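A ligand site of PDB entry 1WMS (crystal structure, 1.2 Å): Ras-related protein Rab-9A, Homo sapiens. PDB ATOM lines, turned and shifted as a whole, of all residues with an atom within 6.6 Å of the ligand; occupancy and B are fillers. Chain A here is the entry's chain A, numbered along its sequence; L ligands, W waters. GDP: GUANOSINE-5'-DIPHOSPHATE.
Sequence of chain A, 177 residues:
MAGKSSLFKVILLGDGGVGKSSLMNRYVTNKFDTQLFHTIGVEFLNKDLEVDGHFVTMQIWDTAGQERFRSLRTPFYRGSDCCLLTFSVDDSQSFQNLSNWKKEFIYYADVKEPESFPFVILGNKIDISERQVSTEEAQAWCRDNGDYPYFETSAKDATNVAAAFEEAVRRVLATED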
ATOM      1  N   GLY A  14      13.336 -26.606  -3.122  1.00  0.00           N
ATOM      2  CA  GLY A  14      14.592 -27.325  -3.095  1.00  0.00           C
ATOM      3  C   GLY A  14      14.812 -27.967  -1.748  1.00  0.00           C
ATOM      4  O   GLY A  14      14.116 -27.605  -0.792  1.00  0.00           O
ATOM      5  N   ASP A  15      15.766 -28.865  -1.658  1.00  0.00           N
ATOM      6  CA  ASP A  15      15.994 -29.601  -0.451  1.00  0.00           C
ATOM      7  C   ASP A  15      16.302 -28.672   0.720  1.00  0.00           C
ATOM      8  O   ASP A  15      16.829 -27.571   0.606  1.00  0.00           O
ATOM      9  CB  ASP A  15      17.171 -30.568  -0.590  1.00  0.00           C
ATOM     10  CG  ASP A  15      16.871 -31.807  -1.413  1.00  0.00           C
ATOM     11  OD1 ASP A  15      15.728 -31.905  -1.911  1.00  0.00           O
ATOM     12  OD2 ASP A  15      17.835 -32.611  -1.506  1.00  0.00           O
ATOM     13  N   GLY A  16      15.983 -29.163   1.911  1.00  0.00           N
ATOM     14  CA  GLY A  16      16.396 -28.457   3.109  1.00  0.00           C
ATOM     15  C   GLY A  16      17.905 -28.211   3.135  1.00  0.00           C
ATOM     16  O   GLY A  16      18.697 -29.087   2.798  1.00  0.00           O
ATOM     17  N   GLY A  17      18.270 -26.983   3.511  1.00  0.00           N
ATOM     18  CA  GLY A  17      19.659 -26.647   3.693  1.00  0.00           C
ATOM     19  C   GLY A  17      20.347 -26.089   2.478  1.00  0.00           C
ATOM     20  O   GLY A  17      21.545 -25.738   2.600  1.00  0.00           O
ATOM     21  N   VAL A  18      19.710 -26.029   1.343  1.00  0.00           N
ATOM     22  CA  VAL A  18      20.408 -25.563   0.143  1.00  0.00           C
ATOM     23  C   VAL A  18      20.590 -24.053   0.115  1.00  0.00           C
ATOM     24  O   VAL A  18      21.482 -23.593  -0.634  1.00  0.00           O
ATOM     25  CB  VAL A  18      19.721 -26.015  -1.157  1.00  0.00           C
ATOM     26  CG1 VAL A  18      19.677 -27.531  -1.279  1.00  0.00           C
ATOM     27  CG2 VAL A  18      18.325 -25.445  -1.355  1.00  0.00           C
ATOM     28  N   GLY A  19      19.825 -23.321   0.906  1.00  0.00           N
ATOM     29  CA  GLY A  19      20.031 -21.886   0.992  1.00  0.00           C
ATOM     30  C   GLY A  19      18.840 -21.086   0.544  1.00  0.00           C
ATOM     31  O   GLY A  19      19.008 -19.864   0.275  1.00  0.00           O
ATOM     32  N   LYS A  20      17.651 -21.624   0.464  1.00  0.00           N
ATOM     33  CA  LYS A  20      16.462 -20.893  -0.006  1.00  0.00           C
ATOM     34  C   LYS A  20      16.166 -19.676   0.837  1.00  0.00           C
ATOM     35  O   LYS A  20      15.980 -18.534   0.335  1.00  0.00           O
ATOM     36  CB  LYS A  20      15.229 -21.814  -0.050  1.00  0.00           C
ATOM     37  CG  LYS A  20      15.447 -23.001  -1.002  1.00  0.00           C
ATOM     38  CD  LYS A  20      14.272 -23.946  -1.000  1.00  0.00           C
ATOM     39  CE  LYS A  20      13.843 -24.532   0.327  1.00  0.00           C
ATOM     40  NZ  LYS A  20      14.901 -25.361   0.955  1.00  0.00           N
ATOM     41  N   SER A  21      16.065 -19.856   2.140  1.00  0.00           N
ATOM     42  CA  SER A  21      15.789 -18.732   2.998  1.00  0.00           C
ATOM     43  C   SER A  21      16.875 -17.679   2.896  1.00  0.00           C
ATOM     44  O   SER A  21      16.589 -16.480   2.881  1.00  0.00           O
ATOM     45  CB  SER A  21      15.703 -19.235   4.454  1.00  0.00           C
ATOM     46  OG  SER A  21      15.496 -18.117   5.281  1.00  0.00           O
ATOM     47  N   SER A  22      18.112 -18.128   2.910  1.00  0.00           N
ATOM     48  CA  SER A  22      19.243 -17.210   2.834  1.00  0.00           C
ATOM     49  C   SER A  22      19.230 -16.436   1.513  1.00  0.00           C
ATOM     50  O   SER A  22      19.538 -15.245   1.518  1.00  0.00           O
ATOM     51  CB  SER A  22      20.557 -17.966   2.973  1.00  0.00           C
ATOM     52  OG  SER A  22      20.648 -18.581   4.256  1.00  0.00           O
ATOM     53  N   LEU A  23      18.880 -17.045   0.421  1.00  0.00           N
ATOM     54  CA  LEU A  23      18.815 -16.372  -0.869  1.00  0.00           C
ATOM     55  C   LEU A  23      17.771 -15.289  -0.893  1.00  0.00           C
ATOM     56  O   LEU A  23      18.016 -14.178  -1.341  1.00  0.00           O
ATOM     57  CB  LEU A  23      18.567 -17.401  -1.962  1.00  0.00           C
ATOM     58  CG  LEU A  23      19.767 -18.229  -2.411  1.00  0.00           C
ATOM     59  CD1 LEU A  23      19.356 -19.477  -3.165  1.00  0.00           C
ATOM     60  CD2 LEU A  23      20.715 -17.365  -3.224  1.00  0.00           C
ATOM     61  N   PHE A  32      23.430 -11.405   5.080  1.00  0.00           N
ATOM     62  CA  PHE A  32      23.551 -12.821   5.298  1.00  0.00           C
ATOM     63  C   PHE A  32      24.063 -13.026   6.718  1.00  0.00           C
ATOM     64  O   PHE A  32      25.071 -12.432   7.102  1.00  0.00           O
ATOM     65  CB  PHE A  32      24.530 -13.431   4.286  1.00  0.00           C
ATOM     66  CG  PHE A  32      24.845 -14.915   4.526  1.00  0.00           C
ATOM     67  CD1 PHE A  32      24.037 -15.860   3.942  1.00  0.00           C
ATOM     68  CD2 PHE A  32      25.921 -15.334   5.308  1.00  0.00           C
ATOM     69  CE1 PHE A  32      24.269 -17.189   4.142  1.00  0.00           C
ATOM     70  CE2 PHE A  32      26.172 -16.668   5.498  1.00  0.00           C
ATOM     71  CZ  PHE A  32      25.347 -17.585   4.896  1.00  0.00           C
ATOM     72  N   ASP A  33      23.442 -13.930   7.446  1.00  0.00           N
ATOM     73  CA  ASP A  33      23.959 -14.265   8.778  1.00  0.00           C
ATOM     74  C   ASP A  33      23.557 -15.683   9.111  1.00  0.00           C
ATOM     75  O   ASP A  33      22.368 -15.968   9.261  1.00  0.00           O
ATOM     76  CB  ASP A  33      23.398 -13.257   9.774  1.00  0.00           C
ATOM     77  CG  ASP A  33      23.996 -13.323  11.162  1.00  0.00           C
ATOM     78  OD1 ASP A  33      24.438 -14.413  11.587  1.00  0.00           O
ATOM     79  OD2 ASP A  33      24.032 -12.272  11.851  1.00  0.00           O
ATOM     80  N   THR A  34      24.500 -16.603   9.301  1.00  0.00           N
ATOM     81  CA  THR A  34      24.108 -17.951   9.739  1.00  0.00           C
ATOM     82  C   THR A  34      23.691 -17.920  11.214  1.00  0.00           C
ATOM     83  O   THR A  34      23.135 -18.938  11.680  1.00  0.00           O
ATOM     84  CB  THR A  34      25.262 -18.925   9.458  1.00  0.00           C
ATOM     85  OG1 THR A  34      24.834 -20.286   9.360  1.00  0.00           O
ATOM     86  CG2 THR A  34      26.255 -18.864  10.606  1.00  0.00           C
ATOM     87  N   ASP A  62       8.778 -19.011   0.232  1.00  0.00           N
ATOM     88  CA  ASP A  62       9.536 -20.158   0.650  1.00  0.00           C
ATOM     89  C   ASP A  62       8.514 -21.048   1.380  1.00  0.00           C
ATOM     90  O   ASP A  62       8.161 -20.694   2.511  1.00  0.00           O
ATOM     91  CB  ASP A  62      10.495 -19.951   1.749  1.00  0.00           C
ATOM     92  CG  ASP A  62      11.607 -20.894   2.032  1.00  0.00           C
ATOM     93  OD1 ASP A  62      11.312 -22.037   1.691  1.00  0.00           O
ATOM     94  OD2 ASP A  62      12.572 -20.517   2.666  1.00  0.00           O
ATOM     95  N   ALA A  64       8.656 -24.265   2.220  1.00  0.00           N
ATOM     96  CA  ALA A  64       9.240 -25.287   3.046  1.00  0.00           C
ATOM     97  C   ALA A  64       8.919 -25.035   4.527  1.00  0.00           C
ATOM     98  O   ALA A  64       9.810 -24.785   5.346  1.00  0.00           O
ATOM     99  CB  ALA A  64      10.751 -25.352   2.899  1.00  0.00           C
ATOM    100  N   THR A  86      16.175 -24.854  -6.520  1.00  0.00           N
ATOM    101  CA  THR A  86      17.449 -24.588  -5.898  1.00  0.00           C
ATOM    102  C   THR A  86      18.146 -25.831  -5.398  1.00  0.00           C
ATOM    103  O   THR A  86      17.481 -26.672  -4.760  1.00  0.00           O
ATOM    104  CB  THR A  86      17.196 -23.631  -4.702  1.00  0.00           C
ATOM    105  OG1 THR A  86      16.435 -22.511  -5.143  1.00  0.00           O
ATOM    106  CG2 THR A  86      18.500 -23.098  -4.157  1.00  0.00           C
ATOM    107  N   ASN A 124      23.418 -23.026  -5.594  1.00  0.00           N
ATOM    108  CA  ASN A 124      23.900 -22.150  -4.540  1.00  0.00           C
ATOM    109  C   ASN A 124      25.141 -22.621  -3.802  1.00  0.00           C
ATOM    110  O   ASN A 124      25.550 -23.780  -3.960  1.00  0.00           O
ATOM    111  CB  ASN A 124      22.737 -21.923  -3.548  1.00  0.00           C
ATOM    112  CG  ASN A 124      22.955 -20.788  -2.609  1.00  0.00           C
ATOM    113  OD1 ASN A 124      23.407 -19.717  -3.002  1.00  0.00           O
ATOM    114  ND2 ASN A 124      22.648 -21.017  -1.336  1.00  0.00           N
ATOM    115  N   LYS A 125      25.740 -21.756  -3.031  1.00  0.00           N
ATOM    116  CA  LYS A 125      26.909 -21.977  -2.216  1.00  0.00           C
ATOM    117  C   LYS A 125      28.179 -22.075  -3.009  1.00  0.00           C
ATOM    118  O   LYS A 125      29.108 -22.779  -2.619  1.00  0.00           O
ATOM    119  CB  LYS A 125      26.756 -23.206  -1.270  1.00  0.00           C
ATOM    120  CG  LYS A 125      25.453 -23.215  -0.497  1.00  0.00           C
ATOM    121  CD  LYS A 125      25.523 -24.180   0.688  1.00  0.00           C
ATOM    122  CE  LYS A 125      24.199 -24.276   1.403  1.00  0.00           C
ATOM    123  NZ  LYS A 125      24.293 -25.128   2.628  1.00  0.00           N
ATOM    124  N   ILE A 126      28.281 -21.283  -4.110  1.00  0.00           N
ATOM    125  CA  ILE A 126      29.482 -21.455  -4.932  1.00  0.00           C
ATOM    126  C   ILE A 126      30.723 -20.862  -4.277  1.00  0.00           C
ATOM    127  O   ILE A 126      31.828 -21.023  -4.807  1.00  0.00           O
ATOM    128  CB  ILE A 126      29.311 -20.826  -6.309  1.00  0.00           C
ATOM    129  CG1 ILE A 126      29.154 -19.299  -6.297  1.00  0.00           C
ATOM    130  CG2 ILE A 126      28.111 -21.514  -6.877  1.00  0.00           C
ATOM    131  CD1 ILE A 126      29.382 -18.790  -7.719  1.00  0.00           C
ATOM    132  N   ASP A 127      30.518 -20.195  -3.126  1.00  0.00           N
ATOM    133  CA  ASP A 127      31.689 -19.781  -2.355  1.00  0.00           C
ATOM    134  C   ASP A 127      32.425 -20.958  -1.719  1.00  0.00           C
ATOM    135  O   ASP A 127      33.548 -20.766  -1.195  1.00  0.00           O
ATOM    136  CB  ASP A 127      31.259 -18.782  -1.267  1.00  0.00           C
ATOM    137  CG  ASP A 127      30.206 -19.424  -0.378  1.00  0.00           C
ATOM    138  OD1 ASP A 127      29.031 -19.458  -0.809  1.00  0.00           O
ATOM    139  OD2 ASP A 127      30.544 -19.894   0.740  1.00  0.00           O
ATOM    140  N   ILE A 128      31.843 -22.167  -1.749  1.00  0.00           N
ATOM    141  CA  ILE A 128      32.488 -23.350  -1.171  1.00  0.00           C
ATOM    142  C   ILE A 128      33.308 -24.013  -2.286  1.00  0.00           C
ATOM    143  O   ILE A 128      32.746 -24.364  -3.329  1.00  0.00           O
ATOM    144  CB  ILE A 128      31.455 -24.321  -0.585  1.00  0.00           C
ATOM    145  CG1 ILE A 128      30.638 -23.630   0.522  1.00  0.00           C
ATOM    146  CG2 ILE A 128      32.085 -25.619  -0.119  1.00  0.00           C
ATOM    147  CD1 ILE A 128      29.537 -24.492   1.060  1.00  0.00           C
ATOM    148  N   THR A 153      25.081 -19.261  -7.650  1.00  0.00           N
ATOM    149  CA  THR A 153      24.805 -18.223  -6.694  1.00  0.00           C
ATOM    150  C   THR A 153      25.547 -18.436  -5.396  1.00  0.00           C
ATOM    151  O   THR A 153      25.926 -19.547  -5.035  1.00  0.00           O
ATOM    152  CB  THR A 153      23.295 -18.071  -6.353  1.00  0.00           C
ATOM    153  OG1 THR A 153      22.783 -19.248  -5.730  1.00  0.00           O
ATOM    154  CG2 THR A 153      22.439 -17.811  -7.567  1.00  0.00           C
ATOM    155  N   SER A 154      25.688 -17.348  -4.648  1.00  0.00           N
ATOM    156  CA  SER A 154      26.074 -17.419  -3.250  1.00  0.00           C
ATOM    157  C   SER A 154      25.289 -16.423  -2.418  1.00  0.00           C
ATOM    158  O   SER A 154      25.466 -15.220  -2.567  1.00  0.00           O
ATOM    159  CB  SER A 154      27.573 -17.167  -3.133  1.00  0.00           C
ATOM    160  OG  SER A 154      27.954 -17.282  -1.743  1.00  0.00           O
ATOM    161  N   ALA A 155      24.399 -16.876  -1.536  1.00  0.00           N
ATOM    162  CA  ALA A 155      23.757 -15.951  -0.607  1.00  0.00           C
ATOM    163  C   ALA A 155      24.792 -15.329   0.288  1.00  0.00           C
ATOM    164  O   ALA A 155      24.623 -14.208   0.738  1.00  0.00           O
ATOM    165  CB  ALA A 155      22.688 -16.645   0.205  1.00  0.00           C
ATOM    166  N   LYS A 156      25.878 -16.069   0.578  1.00  0.00           N
ATOM    167  CA  LYS A 156      26.847 -15.586   1.546  1.00  0.00           C
ATOM    168  C   LYS A 156      27.624 -14.395   1.043  1.00  0.00           C
ATOM    169  O   LYS A 156      27.912 -13.423   1.734  1.00  0.00           O
ATOM    170  CB  LYS A 156      27.738 -16.797   1.903  1.00  0.00           C
ATOM    171  CG  LYS A 156      28.763 -16.451   3.001  1.00  0.00           C
ATOM    172  CD  LYS A 156      29.487 -17.723   3.446  1.00  0.00           C
ATOM    173  CE  LYS A 156      30.417 -17.420   4.611  1.00  0.00           C
ATOM    174  NZ  LYS A 156      31.026 -18.728   5.029  1.00  0.00           N
ATOM    175  N   ASP A 157      27.970 -14.268  -0.203  1.00  0.00           N
ATOM    176  CA  ASP A 157      28.765 -13.256  -0.854  1.00  0.00           C
ATOM    177  C   ASP A 157      27.971 -12.469  -1.886  1.00  0.00           C
ATOM    178  O   ASP A 157      28.585 -11.547  -2.442  1.00  0.00           O
ATOM    179  CB  ASP A 157      30.041 -13.853  -1.413  1.00  0.00           C
ATOM    180  CG  ASP A 157      30.097 -14.583  -2.696  1.00  0.00           C
ATOM    181  OD1 ASP A 157      29.116 -14.484  -3.464  1.00  0.00           O
ATOM    182  OD2 ASP A 157      31.183 -15.200  -2.889  1.00  0.00           O
HETATM  183  PB  GDP L   1      17.039 -23.576   3.379  1.00  0.00           P
HETATM  184  O1B GDP L   1      16.743 -24.726   4.288  1.00  0.00           O
HETATM  185  O2B GDP L   1      17.149 -24.000   1.945  1.00  0.00           O
HETATM  186  O3B GDP L   1      16.172 -22.368   3.604  1.00  0.00           O
HETATM  187  O3A GDP L   1      18.582 -23.136   3.764  1.00  0.00           O
HETATM  188  PA  GDP L   1      19.080 -21.933   4.652  1.00  0.00           P
HETATM  189  O1A GDP L   1      18.962 -20.626   3.945  1.00  0.00           O
HETATM  190  O2A GDP L   1      18.526 -22.035   6.014  1.00  0.00           O
HETATM  191  O5' GDP L   1      20.629 -22.206   4.708  1.00  0.00           O
HETATM  192  C5' GDP L   1      21.112 -23.556   5.152  1.00  0.00           C
HETATM  193  C4' GDP L   1      22.467 -23.281   5.727  1.00  0.00           C
HETATM  194  O4' GDP L   1      23.429 -22.976   4.614  1.00  0.00           O
HETATM  195  C3' GDP L   1      22.612 -22.090   6.726  1.00  0.00           C
HETATM  196  O3' GDP L   1      23.708 -22.515   7.644  1.00  0.00           O
HETATM  197  C2' GDP L   1      23.106 -20.964   5.775  1.00  0.00           C
HETATM  198  O2' GDP L   1      23.859 -19.974   6.494  1.00  0.00           O
HETATM  199  C1' GDP L   1      23.968 -21.716   4.839  1.00  0.00           C
HETATM  200  N9  GDP L   1      24.111 -20.982   3.514  1.00  0.00           N
HETATM  201  C8  GDP L   1      22.943 -20.496   2.820  1.00  0.00           C
HETATM  202  N7  GDP L   1      23.454 -19.992   1.638  1.00  0.00           N
HETATM  203  C5  GDP L   1      24.783 -20.171   1.645  1.00  0.00           C
HETATM  204  C6  GDP L   1      25.821 -19.832   0.790  1.00  0.00           C
HETATM  205  O6  GDP L   1      25.573 -19.189  -0.349  1.00  0.00           O
HETATM  206  N1  GDP L   1      27.082 -20.178   1.096  1.00  0.00           N
HETATM  207  C2  GDP L   1      27.304 -20.875   2.220  1.00  0.00           C
HETATM  208  N2  GDP L   1      28.606 -21.118   2.391  1.00  0.00           N
HETATM  209  N3  GDP L   1      26.448 -21.206   3.138  1.00  0.00           N
HETATM  210  C4  GDP L   1      25.268 -20.856   2.838  1.00  0.00           C
HETATM  211  O   HOH W   1      21.864 -17.974   6.520  1.00  0.00           O
HETATM  212  O   HOH W   2      25.587 -24.331   6.790  1.00  0.00           O
HETATM  213  O   HOH W   3      21.529 -25.159   8.406  1.00  0.00           O
HETATM  214  O   HOH W   4      13.844 -25.817   3.508  1.00  0.00           O
HETATM  215  O   HOH W   5      19.235 -23.131   8.416  1.00  0.00           O
HETATM  216  O   HOH W   6      13.611 -22.667   3.564  1.00  0.00           O
HETATM  217  O   HOH W   7      17.707 -25.453   6.690  1.00  0.00           O
HETATM  218  O   HOH W   8      18.329 -19.359   7.201  1.00  0.00           O
HETATM  219  O   HOH W   9      26.516 -23.943   4.200  1.00  0.00           O
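The backbone NH (N) of Gly 19 is in hydrogen-bond range of an oxygen (O2B) of the ligand.
The backbone NH of Ser 22 lies within hydrogen-bond range of an oxygen (O1A) of the ligand (2.8 Å).
O3B of the ligand sits at hydrogen-bond distance from N of Ser 21 (2.9 Å).
The backbone NH of Val 18 is in hydrogen-bond range of an oxygen (O2B) of the ligand, at 3.3 Å.
The backbone NH (N) of Lys 20 sits at hydrogen-bond distance from an oxygen (O2B) of the ligand, 2.8 Å away.
ND2 of Asn 124 sits at hydrogen-bond distance from N7 of the ligand (3.2 Å).
N of Ala 155 lies within hydrogen-bond range of O6 of the ligand (2.9 Å).
The side-chain hydroxyl (OG) of Ser 22 is in hydrogen-bond range of an oxygen (O1A) of the ligand.
N of Gly 17 sits at hydrogen-bond distance from O1B of the ligand, at 2.8 Å.
The side-chain hydroxyl (OG1) of Thr 34 sits at hydrogen-bond distance from an oxygen (O3') of the ligand (3.0 Å).
O6 of the ligand sits at hydrogen-bond distance from N of Lys 156 (3.3 Å).
OG of Ser 154 sits at hydrogen-bond distance from O6 of the ligand (3.4 Å).
The side-chain carboxylate (OD1) of Asp 127 is in hydrogen-bond range of a nitrogen (N1) of the ligand (2.8 Å).
NZ of Lys 125 sits at hydrogen-bond distance from O4' of the ligand.
The side-chain amino group (NZ) of Lys 20 is in salt-bridge range of an oxygen (O2B) of the ligand (2.8 Å).
The backbone NH (N) of Ala 155 sits at hydrogen-bond distance from the side-chain amide oxygen (OD1) of Asn 124, at 3.3 Å.
The backbone NH of Lys 125 is in hydrogen-bond range of the backbone carbonyl oxygen of Thr 153 (3.0 Å).
OD1 of Asn 124 lies within hydrogen-bond range of OG1 of Thr 153 (2.8 Å).
The backbone carbonyl oxygen of Val 18 lies within hydrogen-bond range of the side-chain amide nitrogen of Asn 124 (2.9 Å).
NZ of Lys 20 lies within hydrogen-bond range of O of Gly 14, 3.0 Å away.
OG of Ser 154 lies close to N of Lys 156 (3.3 Å).
O of Asp 15 sits at hydrogen-bond distance from NZ of Lys 20 (3.0 Å).
OD1 of Asp 127 lies within hydrogen-bond range of OG of Ser 154, 2.6 Å away.
O of Asp 15 touches O2B of the ligand, 3.8 Å away.
Gly 16 touches the ligand (C to O1B, 3.9 Å).
CZ of Phe 32 touches O2' of the ligand, 3.2 Å away.
Ile 128 touches the ligand.
Hydrophobic or aromatic side chains that line the ligand: Val 18, Phe 32, Ile 128 and Ala 155.
The nearest printed residue that does not touch the ligand is Asp 62 (4.2 Å).
Water W6 bridges OD2 of Asp 62 and O3B of the ligand.
Water W1 lies within hydrogen-bond range of OG of Ser 22, O2' of the ligand and O of Asp 33.
Water W9 lies within hydrogen-bond range of N3 of the ligand (2.9 Å) and NZ of Lys 125 (3.0 Å).
Water W4 lies within hydrogen-bond range of NZ of Lys 20 (2.8 Å) and O1B of the ligand (3.2 Å).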
